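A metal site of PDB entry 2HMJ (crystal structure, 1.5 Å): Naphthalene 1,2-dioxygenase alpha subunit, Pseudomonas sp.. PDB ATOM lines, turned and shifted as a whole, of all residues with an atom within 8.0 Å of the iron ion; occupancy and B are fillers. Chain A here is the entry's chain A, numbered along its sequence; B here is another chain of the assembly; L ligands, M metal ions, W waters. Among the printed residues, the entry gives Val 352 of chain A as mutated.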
ATOM      1  N   ASN A 201       1.440  25.685  11.968  1.00  0.00           N
ATOM      2  CA  ASN A 201       0.462  25.109  12.862  1.00  0.00           C
ATOM      3  C   ASN A 201       0.304  25.984  14.098  1.00  0.00           C
ATOM      4  O   ASN A 201      -0.823  26.293  14.501  1.00  0.00           O
ATOM      5  CB  ASN A 201       0.886  23.686  13.214  1.00  0.00           C
ATOM      6  CG  ASN A 201      -0.065  23.003  14.177  1.00  0.00           C
ATOM      7  OD1 ASN A 201      -0.964  22.259  13.766  1.00  0.00           O
ATOM      8  ND2 ASN A 201       0.091  23.288  15.453  1.00  0.00           N
ATOM      9  N   PHE A 202       1.432  26.417  14.664  1.00  0.00           N
ATOM     10  CA  PHE A 202       1.418  27.328  15.831  1.00  0.00           C
ATOM     11  C   PHE A 202       0.953  28.730  15.510  1.00  0.00           C
ATOM     12  O   PHE A 202       0.349  29.365  16.365  1.00  0.00           O
ATOM     13  CB  PHE A 202       2.782  27.420  16.517  1.00  0.00           C
ATOM     14  CG  PHE A 202       3.029  26.331  17.499  1.00  0.00           C
ATOM     15  CD1 PHE A 202       3.113  25.014  17.085  1.00  0.00           C
ATOM     16  CD2 PHE A 202       3.183  26.609  18.833  1.00  0.00           C
ATOM     17  CE1 PHE A 202       3.310  23.992  17.991  1.00  0.00           C
ATOM     18  CE2 PHE A 202       3.403  25.589  19.741  1.00  0.00           C
ATOM     19  CZ  PHE A 202       3.475  24.280  19.308  1.00  0.00           C
ATOM     20  N   ASP A 205      -3.371  27.658  13.620  1.00  0.00           N
ATOM     21  CA  ASP A 205      -4.207  26.501  13.458  1.00  0.00           C
ATOM     22  C   ASP A 205      -4.942  26.116  14.727  1.00  0.00           C
ATOM     23  O   ASP A 205      -4.478  25.295  15.532  1.00  0.00           O
ATOM     24  CB  ASP A 205      -3.410  25.318  12.902  1.00  0.00           C
ATOM     25  CG  ASP A 205      -4.325  24.329  12.234  1.00  0.00           C
ATOM     26  OD1 ASP A 205      -5.342  23.952  12.850  1.00  0.00           O
ATOM     27  OD2 ASP A 205      -4.069  23.983  11.062  1.00  0.00           O
ATOM     28  N   HIS A 208      -7.414  22.395  13.994  1.00  0.00           N
ATOM     29  CA  HIS A 208      -6.970  20.990  14.196  1.00  0.00           C
ATOM     30  C   HIS A 208      -7.193  20.490  15.618  1.00  0.00           C
ATOM     31  O   HIS A 208      -7.215  19.276  15.869  1.00  0.00           O
ATOM     32  CB  HIS A 208      -5.470  20.808  13.815  1.00  0.00           C
ATOM     33  CG  HIS A 208      -4.502  21.202  14.895  1.00  0.00           C
ATOM     34  ND1 HIS A 208      -4.288  22.523  15.270  1.00  0.00           N
ATOM     35  CD2 HIS A 208      -3.644  20.453  15.628  1.00  0.00           C
ATOM     36  CE1 HIS A 208      -3.368  22.538  16.226  1.00  0.00           C
ATOM     37  NE2 HIS A 208      -2.959  21.305  16.449  1.00  0.00           N
ATOM     38  N   VAL A 209      -7.318  21.399  16.576  1.00  0.00           N
ATOM     39  CA  VAL A 209      -7.148  21.046  17.986  1.00  0.00           C
ATOM     40  C   VAL A 209      -8.094  19.965  18.454  1.00  0.00           C
ATOM     41  O   VAL A 209      -7.656  18.988  19.047  1.00  0.00           O
ATOM     42  CB  VAL A 209      -7.196  22.277  18.907  1.00  0.00           C
ATOM     43  CG1 VAL A 209      -7.155  21.850  20.407  1.00  0.00           C
ATOM     44  CG2 VAL A 209      -6.039  23.201  18.561  1.00  0.00           C
ATOM     45  N   GLY A 210      -9.372  20.108  18.135  1.00  0.00           N
ATOM     46  CA  GLY A 210     -10.396  19.162  18.608  1.00  0.00           C
ATOM     47  C   GLY A 210     -10.245  17.759  18.051  1.00  0.00           C
ATOM     48  O   GLY A 210     -10.560  16.751  18.711  1.00  0.00           O
ATOM     49  N   THR A 212      -7.198  16.515  16.032  1.00  0.00           N
ATOM     50  CA  THR A 212      -5.814  16.022  16.281  1.00  0.00           C
ATOM     51  C   THR A 212      -5.576  15.652  17.743  1.00  0.00           C
ATOM     52  O   THR A 212      -5.051  14.577  18.030  1.00  0.00           O
ATOM     53  CB  THR A 212      -4.724  17.067  15.851  1.00  0.00           C
ATOM     54  OG1 THR A 212      -4.676  17.183  14.427  1.00  0.00           O
ATOM     55  CG2 THR A 212      -3.327  16.668  16.329  1.00  0.00           C
ATOM     56  N   HIS A 213      -6.000  16.531  18.656  1.00  0.00           N
ATOM     57  CA  HIS A 213      -5.684  16.372  20.069  1.00  0.00           C
ATOM     58  C   HIS A 213      -6.830  15.779  20.868  1.00  0.00           C
ATOM     59  O   HIS A 213      -6.838  15.869  22.100  1.00  0.00           O
ATOM     60  CB  HIS A 213      -5.223  17.716  20.674  1.00  0.00           C
ATOM     61  CG  HIS A 213      -3.950  18.249  20.087  1.00  0.00           C
ATOM     62  ND1 HIS A 213      -2.729  17.630  20.257  1.00  0.00           N
ATOM     63  CD2 HIS A 213      -3.717  19.317  19.293  1.00  0.00           C
ATOM     64  CE1 HIS A 213      -1.798  18.301  19.603  1.00  0.00           C
ATOM     65  NE2 HIS A 213      -2.375  19.341  19.019  1.00  0.00           N
ATOM     66  N   LEU A 307       3.220  29.412  23.080  1.00  0.00           N
ATOM     67  CA  LEU A 307       1.849  29.442  23.586  1.00  0.00           C
ATOM     68  C   LEU A 307       1.936  30.195  24.899  1.00  0.00           C
ATOM     69  O   LEU A 307       2.529  29.686  25.853  1.00  0.00           O
ATOM     70  CB  LEU A 307       1.326  28.026  23.854  1.00  0.00           C
ATOM     71  CG  LEU A 307       1.317  27.019  22.701  1.00  0.00           C
ATOM     72  CD1 LEU A 307       0.749  25.675  23.138  1.00  0.00           C
ATOM     73  CD2 LEU A 307       0.600  27.545  21.437  1.00  0.00           C
ATOM     74  N   VAL A 352       4.140  19.124  25.846  1.00  0.00           N
ATOM     75  CA  VAL A 352       4.680  19.450  24.513  1.00  0.00           C
ATOM     76  C   VAL A 352       6.183  19.235  24.373  1.00  0.00           C
ATOM     77  O   VAL A 352       6.744  19.510  23.294  1.00  0.00           O
ATOM     78  CB  VAL A 352       4.309  20.894  24.075  1.00  0.00           C
ATOM     79  CG1 VAL A 352       2.808  21.033  24.041  1.00  0.00           C
ATOM     80  CG2 VAL A 352       4.929  21.950  24.993  1.00  0.00           C
ATOM     81  N   TRP A 358       0.651  15.752  24.137  1.00  0.00           N
ATOM     82  CA  TRP A 358      -0.036  16.596  23.165  1.00  0.00           C
ATOM     83  C   TRP A 358       0.755  16.723  21.885  1.00  0.00           C
ATOM     84  O   TRP A 358       0.217  16.509  20.833  1.00  0.00           O
ATOM     85  CB  TRP A 358      -0.280  18.024  23.688  1.00  0.00           C
ATOM     86  CG  TRP A 358      -1.302  18.164  24.751  1.00  0.00           C
ATOM     87  CD1 TRP A 358      -1.233  17.690  26.010  1.00  0.00           C
ATOM     88  CD2 TRP A 358      -2.507  18.946  24.672  1.00  0.00           C
ATOM     89  NE1 TRP A 358      -2.337  18.104  26.740  1.00  0.00           N
ATOM     90  CE2 TRP A 358      -3.132  18.864  25.928  1.00  0.00           C
ATOM     91  CE3 TRP A 358      -3.116  19.677  23.651  1.00  0.00           C
ATOM     92  CZ2 TRP A 358      -4.347  19.490  26.197  1.00  0.00           C
ATOM     93  CZ3 TRP A 358      -4.318  20.314  23.916  1.00  0.00           C
ATOM     94  CH2 TRP A 358      -4.919  20.205  25.177  1.00  0.00           C
ATOM     95  N   GLU A 359       2.025  17.095  21.986  1.00  0.00           N
ATOM     96  CA  GLU A 359       2.833  17.279  20.778  1.00  0.00           C
ATOM     97  C   GLU A 359       2.966  15.978  19.969  1.00  0.00           C
ATOM     98  O   GLU A 359       3.047  16.009  18.734  1.00  0.00           O
ATOM     99  CB  GLU A 359       4.202  17.872  21.108  1.00  0.00           C
ATOM    100  CG  GLU A 359       5.024  18.222  19.853  1.00  0.00           C
ATOM    101  CD  GLU A 359       5.522  19.667  19.812  1.00  0.00           C
ATOM    102  OE1 GLU A 359       4.753  20.586  20.146  1.00  0.00           O
ATOM    103  OE2 GLU A 359       6.701  19.881  19.402  1.00  0.00           O
ATOM    104  N   SER A 360       2.933  14.832  20.643  1.00  0.00           N
ATOM    105  CA  SER A 360       2.974  13.552  19.938  1.00  0.00           C
ATOM    106  C   SER A 360       1.808  13.422  18.947  1.00  0.00           C
ATOM    107  O   SER A 360       1.953  12.823  17.878  1.00  0.00           O
ATOM    108  CB  SER A 360       2.963  12.387  20.942  1.00  0.00           C
ATOM    109  OG  SER A 360       1.668  12.080  21.427  1.00  0.00           O
ATOM    110  N   ASP A 361       0.645  13.983  19.306  1.00  0.00           N
ATOM    111  CA  ASP A 361      -0.534  13.930  18.427  1.00  0.00           C
ATOM    112  C   ASP A 361      -0.261  14.605  17.080  1.00  0.00           C
ATOM    113  O   ASP A 361      -0.896  14.266  16.080  1.00  0.00           O
ATOM    114  CB  ASP A 361      -1.725  14.687  19.042  1.00  0.00           C
ATOM    115  CG  ASP A 361      -2.179  14.165  20.440  1.00  0.00           C
ATOM    116  OD1 ASP A 361      -1.972  12.967  20.773  1.00  0.00           O
ATOM    117  OD2 ASP A 361      -2.789  14.970  21.187  1.00  0.00           O
ATOM    118  N   ASP A 362       0.636  15.592  17.071  1.00  0.00           N
ATOM    119  CA  ASP A 362       0.908  16.404  15.872  1.00  0.00           C
ATOM    120  C   ASP A 362       1.950  15.772  14.943  1.00  0.00           C
ATOM    121  O   ASP A 362       2.084  16.190  13.785  1.00  0.00           O
ATOM    122  CB  ASP A 362       1.463  17.765  16.276  1.00  0.00           C
ATOM    123  CG  ASP A 362       0.447  18.689  16.863  1.00  0.00           C
ATOM    124  OD1 ASP A 362      -0.505  19.023  16.156  1.00  0.00           O
ATOM    125  OD2 ASP A 362       0.632  19.126  18.017  1.00  0.00           O
ATOM    126  N   ASN A 363       2.710  14.809  15.440  1.00  0.00           N
ATOM    127  CA  ASN A 363       3.889  14.282  14.713  1.00  0.00           C
ATOM    128  C   ASN A 363       3.556  13.809  13.309  1.00  0.00           C
ATOM    129  O   ASN A 363       4.190  14.207  12.341  1.00  0.00           O
ATOM    130  CB  ASN A 363       4.506  13.061  15.436  1.00  0.00           C
ATOM    131  CG  ASN A 363       5.343  13.412  16.669  1.00  0.00           C
ATOM    132  OD1 ASN A 363       5.699  12.506  17.467  1.00  0.00           O
ATOM    133  ND2 ASN A 363       5.702  14.700  16.843  1.00  0.00           N
ATOM    134  N   ASN A 365       0.926  14.297  11.501  1.00  0.00           N
ATOM    135  CA  ASN A 365       0.394  15.413  10.699  1.00  0.00           C
ATOM    136  C   ASN A 365       1.528  16.163  10.011  1.00  0.00           C
ATOM    137  O   ASN A 365       1.517  16.357   8.787  1.00  0.00           O
ATOM    138  CB  ASN A 365      -0.384  16.408  11.578  1.00  0.00           C
ATOM    139  CG  ASN A 365      -1.647  15.823  12.176  1.00  0.00           C
ATOM    140  OD1 ASN A 365      -2.190  14.845  11.692  1.00  0.00           O
ATOM    141  ND2 ASN A 365      -2.131  16.452  13.246  1.00  0.00           N
ATOM    142  N   MET A 366       2.504  16.558  10.785  1.00  0.00           N
ATOM    143  CA  MET A 366       3.546  17.392  10.225  1.00  0.00           C
ATOM    144  C   MET A 366       4.551  16.622   9.403  1.00  0.00           C
ATOM    145  O   MET A 366       5.010  17.118   8.367  1.00  0.00           O
ATOM    146  CB  MET A 366       4.205  18.155  11.320  1.00  0.00           C
ATOM    147  CG  MET A 366       3.215  19.059  11.968  1.00  0.00           C
ATOM    148  SD  MET A 366       4.017  19.912  13.265  1.00  0.00           S
ATOM    149  CE  MET A 366       4.488  18.600  14.359  1.00  0.00           C
ATOM    150  N   TYR B 103      -5.890  15.191  10.736  1.00  0.00           N
ATOM    151  CA  TYR B 103      -5.370  16.524  11.041  1.00  0.00           C
ATOM    152  C   TYR B 103      -6.517  17.457  11.414  1.00  0.00           C
ATOM    153  O   TYR B 103      -6.640  17.824  12.594  1.00  0.00           O
ATOM    154  CB  TYR B 103      -4.518  17.042   9.881  1.00  0.00           C
ATOM    155  CG  TYR B 103      -3.537  18.165  10.198  1.00  0.00           C
ATOM    156  CD1 TYR B 103      -3.621  18.919  11.379  1.00  0.00           C
ATOM    157  CD2 TYR B 103      -2.588  18.537   9.271  1.00  0.00           C
ATOM    158  CE1 TYR B 103      -2.740  19.934  11.646  1.00  0.00           C
ATOM    159  CE2 TYR B 103      -1.694  19.570   9.526  1.00  0.00           C
ATOM    160  CZ  TYR B 103      -1.791  20.269  10.715  1.00  0.00           C
ATOM    161  OH  TYR B 103      -0.893  21.321  10.961  1.00  0.00           O
HETATM  162  C1  LIG L   1      -2.174  22.817  21.022  1.00  0.00           C
HETATM  163  O1  LIG L   1      -2.287  22.350  19.667  1.00  0.00           O
HETATM  164  C2  LIG L   1      -0.932  22.248  21.705  1.00  0.00           C
HETATM  165  O2  LIG L   1       0.096  21.976  20.754  1.00  0.00           O
HETATM  166 FE    FE M   1      -1.418  20.542  17.676  1.00  0.00          FE
HETATM  167  O   HOH W   1      -0.282  22.121  17.899  1.00  0.00           O
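A ring nitrogen (ND1) of His 213 sits close to the backbone carbonyl oxygen (O) of Trp 358 (3.2 Å). A ring nitrogen (ND1) of His 213 is in hydrogen-bond range of the side-chain carboxylate (OD2) of Asp 361, at 2.8 Å. The side-chain amide oxygen (OD1) of Asn 201 sits close to a ring nitrogen (NE2) of His 208, 3.5 Å away. A ring nitrogen (ND1) of His 208 lies within hydrogen-bond range of the backbone carbonyl oxygen (O) of Asp 205 (2.8 Å). The side-chain amide oxygen of Asn 201 sits at hydrogen-bond distance from the side-chain hydroxyl of Tyr 103 of chain B, 3.0 Å away.
Residues that only touch the iron ion: Asn 201. Four residues have an atom within 4 Å of the iron ion: Asn 201, His 208, His 213 and Asp 362.
The iron ion is bound by water W1 (2.0 Å), a ring nitrogen (NE2) of His 213 (2.0 Å), a ring nitrogen (NE2) of His 208 (2.1 Å), the side-chain carboxylate (OD1) of Asp 362 (2.3 Å) and the side-chain carboxylate (OD2) of Asp 362 (2.5 Å). The iron ion has five donor atoms within binding distance. Slightly farther from the iron ion lies O1 of the ligand (2.8 Å).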
